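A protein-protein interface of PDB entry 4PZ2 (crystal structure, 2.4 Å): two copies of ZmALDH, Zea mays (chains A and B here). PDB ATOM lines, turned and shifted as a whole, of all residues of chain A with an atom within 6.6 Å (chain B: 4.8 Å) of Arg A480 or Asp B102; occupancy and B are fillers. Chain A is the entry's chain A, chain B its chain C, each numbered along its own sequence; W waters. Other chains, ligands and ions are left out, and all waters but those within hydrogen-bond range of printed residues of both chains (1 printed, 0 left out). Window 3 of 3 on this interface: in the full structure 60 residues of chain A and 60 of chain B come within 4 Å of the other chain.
The backbone carbonyl oxygen (O) of Val A476 lies within hydrogen-bond range of the side-chain amino group (NZ) of Lys B522 (2.8 Å). O of Val A479 is in hydrogen-bond range of NZ of Lys B522 (2.7 Å). NH2 of Arg A480 is in salt-bridge range of OD1 of Asp B102 (2.8 Å).
The side-chain amide oxygen (OD1) of Asn A454 is in hydrogen-bond range of the backbone NH (N) of Arg A480, at 2.7 Å. O of Gly A459 lies within hydrogen-bond range of N of Gly A482, 3.1 Å away. The backbone NH (N) of Gly A482 is in hydrogen-bond range of the backbone carbonyl oxygen (O) of Leu A460 (2.9 Å). The side-chain carboxylate (OD1) of Asp B102 is in salt-bridge range of the guanidinium group (NH1) of Arg B98. The backbone carbonyl oxygen (O) of Phe B101 is in hydrogen-bond range of the guanidinium group (NH1) of Arg B108 (3.3 Å). O of Asp B102 lies within hydrogen-bond range of NH2 of Arg B108.
Among the printed residues, pairs that only touch across the chains: Arg A477 with Lys B522 (3.7 Å), Arg A480 with Arg B98 (3.6 Å), Arg A480 with Phe B101 (3.7 Å), Ala A481 with Lys B522 (3.2 Å), Gly A482 with Lys B522 (3.5 Å) and Val A484 with Lys B522 (3.9 Å).
Of the printed residues of chain B, Val A479 touches Lys B522 (2.7 Å). Printed residues of chain B within 4 Å of Arg A477: Lys B522. Arg A501 touches none of the printed residues of chain B. The nearest residue of chain B that does not touch Arg A480 is Lys B522 (4.6 Å). The nearest printed residue of chain B that does not touch Val A476 is Phe B101 (11.9 Å).
Hydrophobic or aromatic side chains of chain A that line the printed part of chain B: Val A484. Along chain A the printed residues that touch a printed residue of chain B span positions 476 to 484. Among the printed residues, 9 pairs touch across the chains. Among the printed residues, Asp or Glu carboxylates within 4 Å of a Lys or Arg side-chain nitrogen of the other chain: Arg A480 with Asp B102 (2.8 Å).
No position is printed for both chains. Of the 9 pairs that touch across the chains among the printed residues, none has its exchanged pair printed and touching as well.
Water W1 lies within hydrogen-bond range of OD2 of Asp B102 (2.5 Å) and NH1 of Arg A480 (2.8 Å).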
ATOM      1  N   ILE A 450     -20.513  17.011  -1.121  1.00  0.00           N
ATOM      2  CA  ILE A 450     -21.471  16.017  -1.625  1.00  0.00           C
ATOM      3  C   ILE A 450     -20.762  14.844  -2.310  1.00  0.00           C
ATOM      4  O   ILE A 450     -21.034  13.683  -1.980  1.00  0.00           O
ATOM      5  CB  ILE A 450     -22.572  16.673  -2.515  1.00  0.00           C
ATOM      6  CG1 ILE A 450     -23.532  17.523  -1.649  1.00  0.00           C
ATOM      7  CG2 ILE A 450     -23.348  15.622  -3.348  1.00  0.00           C
ATOM      8  CD1 ILE A 450     -24.396  18.600  -2.413  1.00  0.00           C
ATOM      9  N   ALA A 453     -18.654  12.891   0.242  1.00  0.00           N
ATOM     10  CA  ALA A 453     -19.550  12.133   1.124  1.00  0.00           C
ATOM     11  C   ALA A 453     -20.001  10.842   0.408  1.00  0.00           C
ATOM     12  O   ALA A 453     -20.029   9.774   1.024  1.00  0.00           O
ATOM     13  CB  ALA A 453     -20.762  12.977   1.496  1.00  0.00           C
ATOM     14  N   ASN A 454     -20.283  10.947  -0.909  1.00  0.00           N
ATOM     15  CA  ASN A 454     -20.721   9.849  -1.756  1.00  0.00           C
ATOM     16  C   ASN A 454     -19.602   8.937  -2.240  1.00  0.00           C
ATOM     17  O   ASN A 454     -19.885   7.859  -2.762  1.00  0.00           O
ATOM     18  CB  ASN A 454     -21.544  10.374  -2.918  1.00  0.00           C
ATOM     19  CG  ASN A 454     -22.947  10.770  -2.549  1.00  0.00           C
ATOM     20  OD1 ASN A 454     -23.616  10.149  -1.713  1.00  0.00           O
ATOM     21  ND2 ASN A 454     -23.438  11.803  -3.193  1.00  0.00           N
ATOM     22  N   THR A 456     -17.825   6.425  -1.477  1.00  0.00           N
ATOM     23  CA  THR A 456     -17.828   5.234  -0.632  1.00  0.00           C
ATOM     24  C   THR A 456     -18.703   4.181  -1.305  1.00  0.00           C
ATOM     25  O   THR A 456     -19.578   4.525  -2.105  1.00  0.00           O
ATOM     26  CB  THR A 456     -18.304   5.594   0.824  1.00  0.00           C
ATOM     27  OG1 THR A 456     -18.247   4.436   1.666  1.00  0.00           O
ATOM     28  CG2 THR A 456     -19.723   6.230   0.878  1.00  0.00           C
ATOM     29  N   TYR A 458     -20.403   2.262   0.604  1.00  0.00           N
ATOM     30  CA  TYR A 458     -21.412   2.317   1.653  1.00  0.00           C
ATOM     31  C   TYR A 458     -22.446   3.433   1.452  1.00  0.00           C
ATOM     32  O   TYR A 458     -22.312   4.249   0.544  1.00  0.00           O
ATOM     33  CB  TYR A 458     -20.713   2.469   3.024  1.00  0.00           C
ATOM     34  CG  TYR A 458     -19.846   1.292   3.408  1.00  0.00           C
ATOM     35  CD1 TYR A 458     -20.401   0.033   3.634  1.00  0.00           C
ATOM     36  CD2 TYR A 458     -18.475   1.446   3.613  1.00  0.00           C
ATOM     37  CE1 TYR A 458     -19.615  -1.045   4.043  1.00  0.00           C
ATOM     38  CE2 TYR A 458     -17.679   0.374   4.027  1.00  0.00           C
ATOM     39  CZ  TYR A 458     -18.257  -0.870   4.243  1.00  0.00           C
ATOM     40  OH  TYR A 458     -17.496  -1.932   4.665  1.00  0.00           O
ATOM     41  N   GLY A 459     -23.464   3.445   2.304  1.00  0.00           N
ATOM     42  CA  GLY A 459     -24.537   4.437   2.277  1.00  0.00           C
ATOM     43  C   GLY A 459     -25.563   4.193   3.362  1.00  0.00           C
ATOM     44  O   GLY A 459     -26.758   4.095   3.074  1.00  0.00           O
ATOM     45  N   LEU A 460     -25.097   4.042   4.619  1.00  0.00           N
ATOM     46  CA  LEU A 460     -25.965   3.823   5.765  1.00  0.00           C
ATOM     47  C   LEU A 460     -26.460   5.179   6.334  1.00  0.00           C
ATOM     48  O   LEU A 460     -27.623   5.537   6.126  1.00  0.00           O
ATOM     49  CB  LEU A 460     -25.255   2.930   6.830  1.00  0.00           C
ATOM     50  CG  LEU A 460     -26.121   2.390   7.990  1.00  0.00           C
ATOM     51  CD1 LEU A 460     -27.353   1.632   7.482  1.00  0.00           C
ATOM     52  CD2 LEU A 460     -25.290   1.568   8.940  1.00  0.00           C
ATOM     53  N   VAL A 475     -27.806  19.055   0.320  1.00  0.00           N
ATOM     54  CA  VAL A 475     -26.930  17.987   0.821  1.00  0.00           C
ATOM     55  C   VAL A 475     -27.757  16.734   1.162  1.00  0.00           C
ATOM     56  O   VAL A 475     -27.413  15.639   0.699  1.00  0.00           O
ATOM     57  CB  VAL A 475     -26.050  18.479   1.998  1.00  0.00           C
ATOM     58  CG1 VAL A 475     -25.255  17.334   2.626  1.00  0.00           C
ATOM     59  CG2 VAL A 475     -25.120  19.591   1.541  1.00  0.00           C
ATOM     60  N   VAL A 476     -28.859  16.908   1.939  1.00  0.00           N
ATOM     61  CA  VAL A 476     -29.771  15.838   2.323  1.00  0.00           C
ATOM     62  C   VAL A 476     -30.220  15.011   1.096  1.00  0.00           C
ATOM     63  O   VAL A 476     -30.172  13.768   1.130  1.00  0.00           O
ATOM     64  CB  VAL A 476     -30.988  16.400   3.125  1.00  0.00           C
ATOM     65  CG1 VAL A 476     -32.173  15.438   3.111  1.00  0.00           C
ATOM     66  CG2 VAL A 476     -30.588  16.744   4.555  1.00  0.00           C
ATOM     67  N   ARG A 477     -30.629  15.708   0.014  1.00  0.00           N
ATOM     68  CA  ARG A 477     -31.153  15.088  -1.199  1.00  0.00           C
ATOM     69  C   ARG A 477     -30.109  14.561  -2.143  1.00  0.00           C
ATOM     70  O   ARG A 477     -30.454  13.805  -3.041  1.00  0.00           O
ATOM     71  CB  ARG A 477     -32.096  16.054  -1.914  1.00  0.00           C
ATOM     72  CG  ARG A 477     -33.401  16.339  -1.150  1.00  0.00           C
ATOM     73  CD  ARG A 477     -34.173  17.465  -1.811  1.00  0.00           C
ATOM     74  NE  ARG A 477     -34.797  17.036  -3.070  1.00  0.00           N
ATOM     75  CZ  ARG A 477     -36.049  16.594  -3.180  1.00  0.00           C
ATOM     76  NH1 ARG A 477     -36.851  16.577  -2.120  1.00  0.00           N
ATOM     77  NH2 ARG A 477     -36.522  16.208  -4.359  1.00  0.00           N
ATOM     78  N   SER A 478     -28.832  14.967  -1.967  1.00  0.00           N
ATOM     79  CA  SER A 478     -27.720  14.578  -2.827  1.00  0.00           C
ATOM     80  C   SER A 478     -26.846  13.455  -2.260  1.00  0.00           C
ATOM     81  O   SER A 478     -26.223  12.726  -3.044  1.00  0.00           O
ATOM     82  CB  SER A 478     -26.875  15.795  -3.182  1.00  0.00           C
ATOM     83  OG  SER A 478     -27.655  16.857  -3.708  1.00  0.00           O
ATOM     84  N   VAL A 479     -26.795  13.308  -0.914  1.00  0.00           N
ATOM     85  CA  VAL A 479     -26.025  12.242  -0.255  1.00  0.00           C
ATOM     86  C   VAL A 479     -26.801  10.911  -0.305  1.00  0.00           C
ATOM     87  O   VAL A 479     -27.874  10.818   0.268  1.00  0.00           O
ATOM     88  CB  VAL A 479     -25.539  12.623   1.180  1.00  0.00           C
ATOM     89  CG1 VAL A 479     -24.842  11.442   1.866  1.00  0.00           C
ATOM     90  CG2 VAL A 479     -24.601  13.836   1.139  1.00  0.00           C
ATOM     91  N   ARG A 480     -26.244   9.889  -0.986  1.00  0.00           N
ATOM     92  CA  ARG A 480     -26.843   8.554  -1.146  1.00  0.00           C
ATOM     93  C   ARG A 480     -26.697   7.676   0.118  1.00  0.00           C
ATOM     94  O   ARG A 480     -25.926   6.717   0.152  1.00  0.00           O
ATOM     95  CB  ARG A 480     -26.296   7.872  -2.413  1.00  0.00           C
ATOM     96  CG  ARG A 480     -26.815   8.534  -3.677  1.00  0.00           C
ATOM     97  CD  ARG A 480     -26.229   7.911  -4.911  1.00  0.00           C
ATOM     98  NE  ARG A 480     -26.529   8.720  -6.090  1.00  0.00           N
ATOM     99  CZ  ARG A 480     -26.037   8.500  -7.309  1.00  0.00           C
ATOM    100  NH1 ARG A 480     -25.166   7.514  -7.518  1.00  0.00           N
ATOM    101  NH2 ARG A 480     -26.384   9.282  -8.321  1.00  0.00           N
ATOM    102  N   ALA A 481     -27.443   8.039   1.166  1.00  0.00           N
ATOM    103  CA  ALA A 481     -27.462   7.372   2.472  1.00  0.00           C
ATOM    104  C   ALA A 481     -28.904   7.169   2.933  1.00  0.00           C
ATOM    105  O   ALA A 481     -29.795   7.979   2.616  1.00  0.00           O
ATOM    106  CB  ALA A 481     -26.669   8.177   3.501  1.00  0.00           C
ATOM    107  N   GLY A 482     -29.119   6.077   3.661  1.00  0.00           N
ATOM    108  CA  GLY A 482     -30.437   5.721   4.178  1.00  0.00           C
ATOM    109  C   GLY A 482     -31.008   6.676   5.210  1.00  0.00           C
ATOM    110  O   GLY A 482     -32.228   6.829   5.302  1.00  0.00           O
ATOM    111  N   VAL A 484     -30.119  10.666   7.060  1.00  0.00           N
ATOM    112  CA  VAL A 484     -29.384  11.939   7.049  1.00  0.00           C
ATOM    113  C   VAL A 484     -29.852  12.764   8.251  1.00  0.00           C
ATOM    114  O   VAL A 484     -31.028  13.095   8.345  1.00  0.00           O
ATOM    115  CB  VAL A 484     -29.480  12.759   5.723  1.00  0.00           C
ATOM    116  CG1 VAL A 484     -28.502  13.933   5.748  1.00  0.00           C
ATOM    117  CG2 VAL A 484     -29.228  11.886   4.492  1.00  0.00           C
ATOM    118  N   ARG A 501     -28.221   1.883   1.954  1.00  0.00           N
ATOM    119  CA  ARG A 501     -28.243   2.128   0.526  1.00  0.00           C
ATOM    120  C   ARG A 501     -26.865   1.641   0.041  1.00  0.00           C
ATOM    121  O   ARG A 501     -25.926   1.534   0.849  1.00  0.00           O
ATOM    122  CB  ARG A 501     -28.459   3.621   0.220  1.00  0.00           C
ATOM    123  CG  ARG A 501     -28.915   3.857  -1.207  1.00  0.00           C
ATOM    124  CD  ARG A 501     -29.392   5.244  -1.428  1.00  0.00           C
ATOM    125  NE  ARG A 501     -29.588   5.514  -2.853  1.00  0.00           N
ATOM    126  CZ  ARG A 501     -30.099   6.641  -3.329  1.00  0.00           C
ATOM    127  NH1 ARG A 501     -30.510   7.593  -2.498  1.00  0.00           N
ATOM    128  NH2 ARG A 501     -30.241   6.811  -4.638  1.00  0.00           N
ATOM    129  N   LYS A 502     -26.747   1.312  -1.257  1.00  0.00           N
ATOM    130  CA  LYS A 502     -25.497   0.819  -1.846  1.00  0.00           C
ATOM    131  C   LYS A 502     -24.999  -0.440  -1.090  1.00  0.00           C
ATOM    132  O   LYS A 502     -25.825  -1.313  -0.829  1.00  0.00           O
ATOM    133  CB  LYS A 502     -24.453   1.948  -1.927  1.00  0.00           C
ATOM    134  CG  LYS A 502     -24.858   3.107  -2.829  1.00  0.00           C
ATOM    135  CD  LYS A 502     -24.198   4.427  -2.418  1.00  0.00           C
ATOM    136  CE  LYS A 502     -22.721   4.449  -2.709  1.00  0.00           C
ATOM    137  NZ  LYS A 502     -22.149   5.800  -2.563  1.00  0.00           N
ATOM    138  N   ARG B  98     -26.152   4.822 -16.205  1.00  0.00           N
ATOM    139  CA  ARG B  98     -25.485   5.585 -15.153  1.00  0.00           C
ATOM    140  C   ARG B  98     -25.425   7.088 -15.498  1.00  0.00           C
ATOM    141  O   ARG B  98     -25.773   7.919 -14.651  1.00  0.00           O
ATOM    142  CB  ARG B  98     -24.082   5.006 -14.856  1.00  0.00           C
ATOM    143  CG  ARG B  98     -23.295   5.737 -13.743  1.00  0.00           C
ATOM    144  CD  ARG B  98     -24.064   5.939 -12.440  1.00  0.00           C
ATOM    145  NE  ARG B  98     -24.557   4.684 -11.881  1.00  0.00           N
ATOM    146  CZ  ARG B  98     -25.494   4.595 -10.948  1.00  0.00           C
ATOM    147  NH1 ARG B  98     -26.065   5.689 -10.466  1.00  0.00           N
ATOM    148  NH2 ARG B  98     -25.875   3.407 -10.497  1.00  0.00           N
ATOM    149  N   ALA B  99     -25.028   7.424 -16.747  1.00  0.00           N
ATOM    150  CA  ALA B  99     -24.968   8.808 -17.221  1.00  0.00           C
ATOM    151  C   ALA B  99     -26.375   9.437 -17.248  1.00  0.00           C
ATOM    152  O   ALA B  99     -26.534  10.587 -16.829  1.00  0.00           O
ATOM    153  CB  ALA B  99     -24.322   8.877 -18.595  1.00  0.00           C
ATOM    154  N   ALA B 100     -27.400   8.663 -17.679  1.00  0.00           N
ATOM    155  CA  ALA B 100     -28.793   9.109 -17.751  1.00  0.00           C
ATOM    156  C   ALA B 100     -29.367   9.408 -16.371  1.00  0.00           C
ATOM    157  O   ALA B 100     -30.125  10.375 -16.218  1.00  0.00           O
ATOM    158  CB  ALA B 100     -29.640   8.080 -18.473  1.00  0.00           C
ATOM    159  N   PHE B 101     -28.989   8.600 -15.362  1.00  0.00           N
ATOM    160  CA  PHE B 101     -29.442   8.803 -13.989  1.00  0.00           C
ATOM    161  C   PHE B 101     -28.663   9.908 -13.250  1.00  0.00           C
ATOM    162  O   PHE B 101     -29.272  10.770 -12.621  1.00  0.00           O
ATOM    163  CB  PHE B 101     -29.406   7.484 -13.186  1.00  0.00           C
ATOM    164  CG  PHE B 101     -29.987   7.667 -11.810  1.00  0.00           C
ATOM    165  CD1 PHE B 101     -31.366   7.702 -11.620  1.00  0.00           C
ATOM    166  CD2 PHE B 101     -29.160   7.904 -10.713  1.00  0.00           C
ATOM    167  CE1 PHE B 101     -31.905   7.939 -10.352  1.00  0.00           C
ATOM    168  CE2 PHE B 101     -29.697   8.142  -9.445  1.00  0.00           C
ATOM    169  CZ  PHE B 101     -31.067   8.142  -9.271  1.00  0.00           C
ATOM    170  N   ASP B 102     -27.323   9.842 -13.281  1.00  0.00           N
ATOM    171  CA  ASP B 102     -26.462  10.783 -12.579  1.00  0.00           C
ATOM    172  C   ASP B 102     -26.453  12.171 -13.147  1.00  0.00           C
ATOM    173  O   ASP B 102     -26.318  13.116 -12.372  1.00  0.00           O
ATOM    174  CB  ASP B 102     -25.027  10.249 -12.491  1.00  0.00           C
ATOM    175  CG  ASP B 102     -24.787   9.168 -11.450  1.00  0.00           C
ATOM    176  OD1 ASP B 102     -25.775   8.549 -10.989  1.00  0.00           O
ATOM    177  OD2 ASP B 102     -23.612   8.913 -11.126  1.00  0.00           O
ATOM    178  N   HIS B 103     -26.544  12.312 -14.495  1.00  0.00           N
ATOM    179  CA  HIS B 103     -26.443  13.614 -15.169  1.00  0.00           C
ATOM    180  C   HIS B 103     -27.578  13.982 -16.114  1.00  0.00           C
ATOM    181  O   HIS B 103     -27.710  15.156 -16.460  1.00  0.00           O
ATOM    182  CB  HIS B 103     -25.085  13.756 -15.878  1.00  0.00           C
ATOM    183  CG  HIS B 103     -23.915  13.403 -15.009  1.00  0.00           C
ATOM    184  ND1 HIS B 103     -23.543  14.202 -13.936  1.00  0.00           N
ATOM    185  CD2 HIS B 103     -23.108  12.319 -15.047  1.00  0.00           C
ATOM    186  CE1 HIS B 103     -22.522  13.580 -13.368  1.00  0.00           C
ATOM    187  NE2 HIS B 103     -22.226  12.445 -14.002  1.00  0.00           N
ATOM    188  N   GLY B 104     -28.373  12.998 -16.521  1.00  0.00           N
ATOM    189  CA  GLY B 104     -29.479  13.209 -17.446  1.00  0.00           C
ATOM    190  C   GLY B 104     -30.750  13.803 -16.857  1.00  0.00           C
ATOM    191  O   GLY B 104     -30.911  13.915 -15.633  1.00  0.00           O
ATOM    192  N   ARG B 108     -34.486  14.320 -12.990  1.00  0.00           N
ATOM    193  CA  ARG B 108     -34.647  15.753 -12.774  1.00  0.00           C
ATOM    194  C   ARG B 108     -35.981  16.307 -13.276  1.00  0.00           C
ATOM    195  O   ARG B 108     -36.332  17.441 -12.939  1.00  0.00           O
ATOM    196  CB  ARG B 108     -33.457  16.513 -13.372  1.00  0.00           C
ATOM    197  CG  ARG B 108     -32.190  16.322 -12.574  1.00  0.00           C
ATOM    198  CD  ARG B 108     -30.954  16.536 -13.411  1.00  0.00           C
ATOM    199  NE  ARG B 108     -29.740  16.324 -12.620  1.00  0.00           N
ATOM    200  CZ  ARG B 108     -29.159  15.143 -12.417  1.00  0.00           C
ATOM    201  NH1 ARG B 108     -29.666  14.038 -12.963  1.00  0.00           N
ATOM    202  NH2 ARG B 108     -28.066  15.056 -11.670  1.00  0.00           N
ATOM    203  N   LYS B 522     -35.303   7.433   2.110  1.00  0.00           N
ATOM    204  CA  LYS B 522     -34.318   8.177   2.876  1.00  0.00           C
ATOM    205  C   LYS B 522     -34.987   8.850   4.080  1.00  0.00           C
ATOM    206  O   LYS B 522     -35.884   9.662   3.888  1.00  0.00           O
ATOM    207  CB  LYS B 522     -33.646   9.229   1.970  1.00  0.00           C
ATOM    208  CG  LYS B 522     -32.564  10.053   2.669  1.00  0.00           C
ATOM    209  CD  LYS B 522     -31.943  11.072   1.754  1.00  0.00           C
ATOM    210  CE  LYS B 522     -30.863  10.479   0.888  1.00  0.00           C
ATOM    211  NZ  LYS B 522     -30.515  11.383  -0.239  1.00  0.00           N
HETATM  212  O   HOH W   1     -22.966   7.352  -9.258  1.00  0.00           O
